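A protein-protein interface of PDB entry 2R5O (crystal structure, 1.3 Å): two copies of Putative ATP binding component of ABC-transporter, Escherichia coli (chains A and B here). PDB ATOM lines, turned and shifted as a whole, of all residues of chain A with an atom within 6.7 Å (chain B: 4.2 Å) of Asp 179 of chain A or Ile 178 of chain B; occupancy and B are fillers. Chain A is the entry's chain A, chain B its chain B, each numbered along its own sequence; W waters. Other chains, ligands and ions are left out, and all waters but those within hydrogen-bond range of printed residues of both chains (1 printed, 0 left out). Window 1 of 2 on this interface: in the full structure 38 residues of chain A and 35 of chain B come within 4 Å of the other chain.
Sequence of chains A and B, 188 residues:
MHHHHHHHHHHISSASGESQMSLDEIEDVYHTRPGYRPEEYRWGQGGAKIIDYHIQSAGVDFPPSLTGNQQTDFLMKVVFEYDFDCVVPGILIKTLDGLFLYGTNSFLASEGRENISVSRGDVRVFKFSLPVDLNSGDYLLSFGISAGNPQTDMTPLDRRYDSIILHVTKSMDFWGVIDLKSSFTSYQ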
ATOM      1  N   GLY A  68       8.561  13.733 -20.738  1.00  0.00           N
ATOM      2  CA  GLY A  68       8.397  13.748 -19.290  1.00  0.00           C
ATOM      3  C   GLY A  68       9.135  14.921 -18.667  1.00  0.00           C
ATOM      4  O   GLY A  68      10.307  15.167 -18.994  1.00  0.00           O
ATOM      5  N   ASN A  69       8.432  15.655 -17.803  1.00  0.00           N
ATOM      6  CA  ASN A  69       8.950  16.817 -17.036  1.00  0.00           C
ATOM      7  C   ASN A  69       9.001  18.115 -17.793  1.00  0.00           C
ATOM      8  O   ASN A  69       9.285  19.169 -17.217  1.00  0.00           O
ATOM      9  CB  ASN A  69      10.302  16.541 -16.377  1.00  0.00           C
ATOM     10  CG  ASN A  69      10.312  15.257 -15.589  1.00  0.00           C
ATOM     11  OD1 ASN A  69      11.269  14.472 -15.677  1.00  0.00           O
ATOM     12  ND2 ASN A  69       9.232  14.999 -14.853  1.00  0.00           N
ATOM     13  N   PHE A 100      -7.449   9.464 -11.539  1.00  0.00           N
ATOM     14  CA  PHE A 100      -7.508  10.908 -11.698  1.00  0.00           C
ATOM     15  C   PHE A 100      -6.191  11.446 -11.226  1.00  0.00           C
ATOM     16  O   PHE A 100      -5.869  11.429 -10.043  1.00  0.00           O
ATOM     17  CB  PHE A 100      -8.690  11.420 -10.857  1.00  0.00           C
ATOM     18  CG  PHE A 100      -8.998  12.883 -10.951  1.00  0.00           C
ATOM     19  CD1 PHE A 100      -9.765  13.430  -9.951  1.00  0.00           C
ATOM     20  CD2 PHE A 100      -8.587  13.697 -11.994  1.00  0.00           C
ATOM     21  CE1 PHE A 100     -10.089  14.756  -9.970  1.00  0.00           C
ATOM     22  CE2 PHE A 100      -8.917  15.021 -12.015  1.00  0.00           C
ATOM     23  CZ  PHE A 100      -9.672  15.548 -11.019  1.00  0.00           C
ATOM     24  N   LEU A 101      -5.389  11.926 -12.177  1.00  0.00           N
ATOM     25  CA  LEU A 101      -4.020  12.382 -11.892  1.00  0.00           C
ATOM     26  C   LEU A 101      -3.959  13.833 -11.459  1.00  0.00           C
ATOM     27  O   LEU A 101      -3.266  14.158 -10.488  1.00  0.00           O
ATOM     28  CB  LEU A 101      -3.103  12.160 -13.082  1.00  0.00           C
ATOM     29  CG  LEU A 101      -2.884  10.696 -13.451  1.00  0.00           C
ATOM     30  CD1 LEU A 101      -2.209  10.607 -14.826  1.00  0.00           C
ATOM     31  CD2 LEU A 101      -2.055  10.031 -12.397  1.00  0.00           C
ATOM     32  N   TYR A 102      -4.655  14.712 -12.175  1.00  0.00           N
ATOM     33  CA  TYR A 102      -4.591  16.150 -11.869  1.00  0.00           C
ATOM     34  C   TYR A 102      -5.779  16.843 -12.467  1.00  0.00           C
ATOM     35  O   TYR A 102      -6.166  16.534 -13.578  1.00  0.00           O
ATOM     36  CB  TYR A 102      -3.330  16.764 -12.456  1.00  0.00           C
ATOM     37  CG  TYR A 102      -3.195  18.264 -12.277  1.00  0.00           C
ATOM     38  CD1 TYR A 102      -3.060  18.806 -11.022  1.00  0.00           C
ATOM     39  CD2 TYR A 102      -3.186  19.137 -13.376  1.00  0.00           C
ATOM     40  CE1 TYR A 102      -2.887  20.148 -10.831  1.00  0.00           C
ATOM     41  CE2 TYR A 102      -3.007  20.504 -13.199  1.00  0.00           C
ATOM     42  CZ  TYR A 102      -2.837  21.019 -11.921  1.00  0.00           C
ATOM     43  OH  TYR A 102      -2.610  22.362 -11.762  1.00  0.00           O
ATOM     44  N   GLY A 103      -6.360  17.767 -11.728  1.00  0.00           N
ATOM     45  CA  GLY A 103      -7.364  18.662 -12.253  1.00  0.00           C
ATOM     46  C   GLY A 103      -7.234  20.012 -11.625  1.00  0.00           C
ATOM     47  O   GLY A 103      -6.819  20.143 -10.473  1.00  0.00           O
ATOM     48  N   VAL A 132       4.800  18.239 -17.570  1.00  0.00           N
ATOM     49  CA  VAL A 132       4.099  16.976 -17.659  1.00  0.00           C
ATOM     50  C   VAL A 132       4.912  15.918 -16.874  1.00  0.00           C
ATOM     51  O   VAL A 132       5.652  15.095 -17.439  1.00  0.00           O
ATOM     52  CB  VAL A 132       3.822  16.601 -19.110  1.00  0.00           C
ATOM     53  CG1 VAL A 132       3.021  15.306 -19.194  1.00  0.00           C
ATOM     54  CG2 VAL A 132       3.047  17.752 -19.808  1.00  0.00           C
ATOM     55  N   ASP A 133       4.758  15.976 -15.558  1.00  0.00           N
ATOM     56  CA  ASP A 133       5.571  15.186 -14.585  1.00  0.00           C
ATOM     57  C   ASP A 133       4.941  13.768 -14.393  1.00  0.00           C
ATOM     58  O   ASP A 133       4.453  13.419 -13.322  1.00  0.00           O
ATOM     59  CB  ASP A 133       5.690  15.962 -13.254  1.00  0.00           C
ATOM     60  CG  ASP A 133       6.595  17.180 -13.322  1.00  0.00           C
ATOM     61  OD1 ASP A 133       7.358  17.340 -14.282  1.00  0.00           O
ATOM     62  OD2 ASP A 133       6.563  18.020 -12.386  1.00  0.00           O
ATOM     63  N   LEU A 134       4.897  13.026 -15.502  1.00  0.00           N
ATOM     64  CA  LEU A 134       4.256  11.728 -15.631  1.00  0.00           C
ATOM     65  C   LEU A 134       5.207  10.750 -16.278  1.00  0.00           C
ATOM     66  O   LEU A 134       6.147  11.140 -16.988  1.00  0.00           O
ATOM     67  CB  LEU A 134       2.975  11.805 -16.490  1.00  0.00           C
ATOM     68  CG  LEU A 134       1.888  12.757 -15.999  1.00  0.00           C
ATOM     69  CD1 LEU A 134       0.726  12.780 -16.948  1.00  0.00           C
ATOM     70  CD2 LEU A 134       1.416  12.417 -14.612  1.00  0.00           C
ATOM     71  N   ASN A 135       5.001   9.463 -16.015  1.00  0.00           N
ATOM     72  CA  ASN A 135       5.844   8.435 -16.603  1.00  0.00           C
ATOM     73  C   ASN A 135       5.433   8.211 -18.066  1.00  0.00           C
ATOM     74  O   ASN A 135       4.391   8.682 -18.541  1.00  0.00           O
ATOM     75  CB  ASN A 135       5.716   7.130 -15.792  1.00  0.00           C
ATOM     76  CG  ASN A 135       6.998   6.322 -15.752  1.00  0.00           C
ATOM     77  OD1 ASN A 135       7.948   6.620 -16.478  1.00  0.00           O
ATOM     78  ND2 ASN A 135       7.029   5.315 -14.895  1.00  0.00           N
ATOM     79  N   LYS A 170       9.856   9.212 -22.448  1.00  0.00           N
ATOM     80  CA  LYS A 170      11.062   9.393 -21.630  1.00  0.00           C
ATOM     81  C   LYS A 170      12.105   8.391 -22.108  1.00  0.00           C
ATOM     82  O   LYS A 170      11.796   7.409 -22.810  1.00  0.00           O
ATOM     83  CB  LYS A 170      10.767   9.075 -20.157  1.00  0.00           C
ATOM     84  CG  LYS A 170       9.699   9.885 -19.484  1.00  0.00           C
ATOM     85  CD  LYS A 170       9.497   9.454 -18.043  1.00  0.00           C
ATOM     86  CE  LYS A 170      10.703   9.767 -17.188  1.00  0.00           C
ATOM     87  NZ  LYS A 170      10.927  11.236 -17.020  1.00  0.00           N
ATOM     88  N   PHE A 174      10.843   5.750 -14.392  1.00  0.00           N
ATOM     89  CA  PHE A 174      10.914   5.494 -12.981  1.00  0.00           C
ATOM     90  C   PHE A 174       9.789   4.460 -12.707  1.00  0.00           C
ATOM     91  O   PHE A 174       9.194   3.916 -13.665  1.00  0.00           O
ATOM     92  CB  PHE A 174      10.763   6.791 -12.169  1.00  0.00           C
ATOM     93  CG  PHE A 174       9.511   7.580 -12.501  1.00  0.00           C
ATOM     94  CD1 PHE A 174       8.318   7.325 -11.874  1.00  0.00           C
ATOM     95  CD2 PHE A 174       9.545   8.599 -13.451  1.00  0.00           C
ATOM     96  CE1 PHE A 174       7.194   8.031 -12.191  1.00  0.00           C
ATOM     97  CE2 PHE A 174       8.404   9.289 -13.799  1.00  0.00           C
ATOM     98  CZ  PHE A 174       7.240   9.010 -13.158  1.00  0.00           C
ATOM     99  N   VAL A 177       3.683   6.124 -11.837  1.00  0.00           N
ATOM    100  CA  VAL A 177       2.979   6.944 -12.811  1.00  0.00           C
ATOM    101  C   VAL A 177       3.289   8.414 -12.722  1.00  0.00           C
ATOM    102  O   VAL A 177       3.271   9.108 -13.744  1.00  0.00           O
ATOM    103  CB  VAL A 177       1.459   6.654 -12.748  1.00  0.00           C
ATOM    104  CG1 VAL A 177       0.891   6.751 -11.350  1.00  0.00           C
ATOM    105  CG2 VAL A 177       0.690   7.495 -13.728  1.00  0.00           C
ATOM    106  N   ILE A 178       3.561   8.904 -11.513  1.00  0.00           N
ATOM    107  CA  ILE A 178       3.786  10.341 -11.307  1.00  0.00           C
ATOM    108  C   ILE A 178       5.226  10.594 -10.890  1.00  0.00           C
ATOM    109  O   ILE A 178       5.801   9.862 -10.083  1.00  0.00           O
ATOM    110  CB  ILE A 178       2.795  10.898 -10.274  1.00  0.00           C
ATOM    111  CG1 ILE A 178       2.835  10.153  -8.933  1.00  0.00           C
ATOM    112  CG2 ILE A 178       1.387  10.840 -10.854  1.00  0.00           C
ATOM    113  CD1 ILE A 178       2.276  10.926  -7.778  1.00  0.00           C
ATOM    114  N   ASP A 179       5.800  11.661 -11.425  1.00  0.00           N
ATOM    115  CA  ASP A 179       7.187  11.986 -11.161  1.00  0.00           C
ATOM    116  C   ASP A 179       7.282  13.047 -10.069  1.00  0.00           C
ATOM    117  O   ASP A 179       7.008  14.225 -10.324  1.00  0.00           O
ATOM    118  CB  ASP A 179       7.891  12.463 -12.416  1.00  0.00           C
ATOM    119  CG  ASP A 179       9.379  12.499 -12.275  1.00  0.00           C
ATOM    120  OD1 ASP A 179       9.924  12.284 -11.177  1.00  0.00           O
ATOM    121  OD2 ASP A 179      10.027  12.730 -13.314  1.00  0.00           O
ATOM    122  N   LEU A 180       7.692  12.643  -8.869  1.00  0.00           N
ATOM    123  CA  LEU A 180       7.891  13.573  -7.767  1.00  0.00           C
ATOM    124  C   LEU A 180       9.280  14.235  -7.790  1.00  0.00           C
ATOM    125  O   LEU A 180       9.586  15.059  -6.951  1.00  0.00           O
ATOM    126  CB  LEU A 180       7.655  12.869  -6.430  1.00  0.00           C
ATOM    127  CG  LEU A 180       6.190  12.481  -6.207  1.00  0.00           C
ATOM    128  CD1 LEU A 180       6.052  11.627  -4.964  1.00  0.00           C
ATOM    129  CD2 LEU A 180       5.258  13.725  -6.133  1.00  0.00           C
ATOM    130  N   LYS A 181      10.139  13.868  -8.741  1.00  0.00           N
ATOM    131  CA  LYS A 181      11.372  14.614  -9.023  1.00  0.00           C
ATOM    132  C   LYS A 181      12.320  14.685  -7.831  1.00  0.00           C
ATOM    133  O   LYS A 181      12.899  15.720  -7.527  1.00  0.00           O
ATOM    134  CB  LYS A 181      11.042  16.011  -9.568  1.00  0.00           C
ATOM    135  CG  LYS A 181      10.273  15.951 -10.875  1.00  0.00           C
ATOM    136  CD  LYS A 181      10.097  17.291 -11.591  1.00  0.00           C
ATOM    137  CE  LYS A 181      11.419  17.861 -12.103  1.00  0.00           C
ATOM    138  NZ  LYS A 181      11.299  19.290 -12.483  1.00  0.00           N
ATOM    139  N   SER A 182      12.553  13.559  -7.195  1.00  0.00           N
ATOM    140  CA  SER A 182      13.425  13.551  -6.039  1.00  0.00           C
ATOM    141  C   SER A 182      14.853  13.892  -6.417  1.00  0.00           C
ATOM    142  O   SER A 182      15.357  13.469  -7.472  1.00  0.00           O
ATOM    143  CB  SER A 182      13.425  12.164  -5.420  1.00  0.00           C
ATOM    144  OG  SER A 182      14.147  12.124  -4.183  1.00  0.00           O
ATOM    145  N   TYR B 102       5.236   6.362  -7.298  1.00  0.00           N
ATOM    146  CA  TYR B 102       6.558   6.896  -7.622  1.00  0.00           C
ATOM    147  C   TYR B 102       7.642   6.112  -6.938  1.00  0.00           C
ATOM    148  O   TYR B 102       7.645   5.997  -5.716  1.00  0.00           O
ATOM    149  CB  TYR B 102       6.679   8.339  -7.140  1.00  0.00           C
ATOM    150  CG  TYR B 102       8.049   8.973  -7.362  1.00  0.00           C
ATOM    151  CD1 TYR B 102       8.520   9.237  -8.636  1.00  0.00           C
ATOM    152  CD2 TYR B 102       8.887   9.264  -6.290  1.00  0.00           C
ATOM    153  CE1 TYR B 102       9.725   9.808  -8.851  1.00  0.00           C
ATOM    154  CE2 TYR B 102      10.136   9.856  -6.492  1.00  0.00           C
ATOM    155  CZ  TYR B 102      10.546  10.139  -7.783  1.00  0.00           C
ATOM    156  OH  TYR B 102      11.761  10.758  -7.963  1.00  0.00           O
ATOM    157  N   ASP B 133       3.957  16.712  -3.122  1.00  0.00           N
ATOM    158  CA  ASP B 133       2.871  17.402  -3.811  1.00  0.00           C
ATOM    159  C   ASP B 133       1.735  16.458  -4.158  1.00  0.00           C
ATOM    160  O   ASP B 133       1.191  16.474  -5.246  1.00  0.00           O
ATOM    161  CB  ASP B 133       3.402  18.076  -5.061  1.00  0.00           C
ATOM    162  CG  ASP B 133       4.226  19.286  -4.750  1.00  0.00           C
ATOM    163  OD1 ASP B 133       3.824  20.067  -3.844  1.00  0.00           O
ATOM    164  OD2 ASP B 133       5.200  19.539  -5.495  1.00  0.00           O
ATOM    165  N   PHE B 174      -6.005  21.777  -5.415  1.00  0.00           N
ATOM    166  CA  PHE B 174      -5.900  21.076  -6.693  1.00  0.00           C
ATOM    167  C   PHE B 174      -6.660  19.774  -6.540  1.00  0.00           C
ATOM    168  O   PHE B 174      -6.941  19.323  -5.429  1.00  0.00           O
ATOM    169  CB  PHE B 174      -4.439  20.799  -7.089  1.00  0.00           C
ATOM    170  CG  PHE B 174      -3.720  19.868  -6.124  1.00  0.00           C
ATOM    171  CD1 PHE B 174      -3.645  18.485  -6.355  1.00  0.00           C
ATOM    172  CD2 PHE B 174      -3.142  20.371  -4.974  1.00  0.00           C
ATOM    173  CE1 PHE B 174      -2.986  17.652  -5.461  1.00  0.00           C
ATOM    174  CE2 PHE B 174      -2.497  19.518  -4.078  1.00  0.00           C
ATOM    175  CZ  PHE B 174      -2.451  18.180  -4.329  1.00  0.00           C
ATOM    176  N   GLY B 176      -7.012  15.563  -8.040  1.00  0.00           N
ATOM    177  CA  GLY B 176      -6.210  14.446  -8.522  1.00  0.00           C
ATOM    178  C   GLY B 176      -5.083  14.101  -7.582  1.00  0.00           C
ATOM    179  O   GLY B 176      -4.834  14.813  -6.600  1.00  0.00           O
ATOM    180  N   VAL B 177      -4.350  13.048  -7.896  1.00  0.00           N
ATOM    181  CA  VAL B 177      -3.340  12.570  -6.957  1.00  0.00           C
ATOM    182  C   VAL B 177      -2.112  13.461  -6.850  1.00  0.00           C
ATOM    183  O   VAL B 177      -1.508  13.506  -5.785  1.00  0.00           O
ATOM    184  CB  VAL B 177      -3.009  11.099  -7.192  1.00  0.00           C
ATOM    185  CG1 VAL B 177      -2.291  10.908  -8.454  1.00  0.00           C
ATOM    186  CG2 VAL B 177      -2.205  10.539  -6.031  1.00  0.00           C
ATOM    187  N   ILE B 178      -1.711  14.136  -7.928  1.00  0.00           N
ATOM    188  CA  ILE B 178      -0.506  14.974  -7.904  1.00  0.00           C
ATOM    189  C   ILE B 178      -0.807  16.421  -8.309  1.00  0.00           C
ATOM    190  O   ILE B 178      -1.519  16.669  -9.276  1.00  0.00           O
ATOM    191  CB  ILE B 178       0.623  14.411  -8.833  1.00  0.00           C
ATOM    192  CG1 ILE B 178       1.894  15.274  -8.746  1.00  0.00           C
ATOM    193  CG2 ILE B 178       0.136  14.248 -10.263  1.00  0.00           C
ATOM    194  CD1 ILE B 178       3.163  14.703  -9.348  1.00  0.00           C
ATOM    195  N   ASP B 179      -0.234  17.374  -7.595  1.00  0.00           N
ATOM    196  CA  ASP B 179      -0.305  18.772  -7.960  1.00  0.00           C
ATOM    197  C   ASP B 179       0.743  19.055  -9.035  1.00  0.00           C
ATOM    198  O   ASP B 179       1.937  19.153  -8.725  1.00  0.00           O
ATOM    199  CB  ASP B 179      -0.095  19.656  -6.740  1.00  0.00           C
ATOM    200  CG  ASP B 179      -0.313  21.105  -7.025  1.00  0.00           C
ATOM    201  OD1 ASP B 179      -0.703  21.468  -8.167  1.00  0.00           O
ATOM    202  OD2 ASP B 179      -0.079  21.933  -6.093  1.00  0.00           O
ATOM    203  N   LEU B 180       0.313  19.181 -10.291  1.00  0.00           N
ATOM    204  CA  LEU B 180       1.218  19.504 -11.400  1.00  0.00           C
ATOM    205  C   LEU B 180       1.476  21.004 -11.504  1.00  0.00           C
ATOM    206  O   LEU B 180       2.245  21.428 -12.371  1.00  0.00           O
ATOM    207  CB  LEU B 180       0.696  18.931 -12.726  1.00  0.00           C
ATOM    208  CG  LEU B 180       0.649  17.399 -12.781  1.00  0.00           C
ATOM    209  CD1 LEU B 180       0.021  16.924 -14.077  1.00  0.00           C
ATOM    210  CD2 LEU B 180       2.005  16.781 -12.570  1.00  0.00           C
HETATM  211  O   HOH W   1       4.869  20.262 -11.333  1.00  0.00           O
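O of Phe 100 of chain A lies within hydrogen-bond range of N of Val 177 of chain B (3.1 Å).
The backbone NH (N) of Val 177 of chain B lies within hydrogen-bond range of the backbone carbonyl oxygen (O) of Leu 101 of chain A, 3.0 Å away.
The backbone carbonyl oxygen of Leu 101 of chain A is in hydrogen-bond range of the backbone NH of Ile 178 of chain B (3.0 Å).
The backbone NH (N) of Ser 182 of chain A lies within hydrogen-bond range of the side-chain hydroxyl (OH) of Tyr 102 of chain B, at 3.0 Å.
The side-chain amide nitrogen (ND2) of Asn 69 of chain A is in hydrogen-bond range of the side-chain carboxylate (OD1) of Asp 133 of chain A (3.1 Å).
OD2 of Asp 179 of chain A sits at hydrogen-bond distance from ND2 of Asn 69 of chain A (2.9 Å).
The backbone carbonyl oxygen (O) of Asp 133 of chain A lies within hydrogen-bond range of the backbone NH (N) of Asp 179 of chain A (2.9 Å).
The side-chain amide nitrogen (ND2) of Asn 135 of chain A sits at hydrogen-bond distance from the backbone carbonyl oxygen (O) of Phe 174 of chain A (2.9 Å).
The side-chain carboxylate (OD1) of Asp 179 of chain A is in hydrogen-bond range of the backbone NH (N) of Lys 181 of chain A, 2.9 Å away.
The backbone carbonyl oxygen (O) of Asp 133 of chain B sits at hydrogen-bond distance from the backbone NH (N) of Asp 179 of chain B.
Among the printed residues, pairs that only touch across the chains: Ile 178 of chain A with Tyr 102 of chain B (3.1 Å), Tyr 102 of chain A with Ile 178 of chain B (3.2 Å), Tyr 102 of chain A with Leu 180 of chain B (3.4 Å), Phe 100 of chain A with Gly 176 of chain B (3.4 Å), Asp 179 of chain A with Tyr 102 of chain B (3.4 Å), Leu 101 of chain A with Gly 176 of chain B (3.4 Å), Leu 180 of chain A with Tyr 102 of chain B (3.5 Å), Lys 181 of chain A with Tyr 102 of chain B (3.6 Å), Ile 178 of chain A with Ile 178 of chain B (3.7 Å), Tyr 102 of chain A with Asp 179 of chain B (3.7 Å), Phe 174 of chain A with Tyr 102 of chain B (3.8 Å), Asp 133 of chain A with Leu 180 of chain B (3.8 Å), Gly 103 of chain A with Phe 174 of chain B (3.95 Å), Leu 180 of chain A with Ile 178 of chain B (3.96 Å), Tyr 102 of chain A with Gly 176 of chain B (3.98 Å) and Asp 179 of chain A with Ile 178 of chain B (3.996 Å).
Of the printed residues of chain A, Ile 178 of chain B touches Leu 101 (3.0 Å), Tyr 102 (3.2 Å), Ile 178 (3.7 Å), Asp 179 (3.996 Å) and Leu 180 (3.96 Å).
Of the printed residues of chain B, Leu 101 of chain A touches Gly 176, Val 177 and Ile 178.
Printed residues of chain B within 4 Å of Leu 180 of chain A: Tyr 102 (3.5 Å) and Ile 178 (3.96 Å).
Leu 134 of chain A touches none of the printed residues of chain B.
The nearest printed residue of chain B that does not touch Phe 174 of chain A is Ile 178 of chain B (8.0 Å).
Printed residues of chain B that touch a printed residue of chain A: Tyr 102, Phe 174, Gly 176, Val 177, Ile 178, Asp 179 and Leu 180.
Hydrophobic or aromatic side chains of chain B that line the printed part of chain A: Tyr 102, Val 177, Ile 178 and Leu 180.
Of the 18 printed residues of chain A, 11 touch a printed residue of chain B.
Hydrophobic or aromatic side chains of chain A within 4 Å of the printed part of chain B: Phe 100, Tyr 102, Phe 174, Ile 178 and Leu 180.
Among the printed residues, 20 pairs touch across the chains.
Among the printed residues, no Asp or Glu carboxylate lies within 4 Å of a Lys or Arg side-chain nitrogen of the other chain.
Tyr 102 of chain A touches Asp 179 of chain B, and with the chains exchanged Asp 179 of chain A touches Tyr 102 of chain B.
Asp 133 of chain A touches Leu 180 of chain B, but with the chains exchanged Leu 180 of chain A does not touch Asp 133 of chain B (4.4 Å).
Phe 174 of chain A touches Tyr 102 of chain B, but with the chains exchanged Tyr 102 of chain A does not touch Phe 174 of chain B (4.1 Å).
Leu 180 of chain A touches Ile 178 of chain B, but with the chains exchanged Ile 178 of chain A does not touch Leu 180 of chain B (6.2 Å).
Positions printed for both chains: 102, 133, 174, 177, 178, 179 and 180.
Of the 20 pairs that touch across the chains among the printed residues, 7 have their exchanged pair printed and touching as well.
Water W1 lies within hydrogen-bond range of the side-chain carboxylate of Asp 133 of chain A (3.0 Å) and the backbone carbonyl oxygen of Leu 180 of chain B (3.1 Å).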
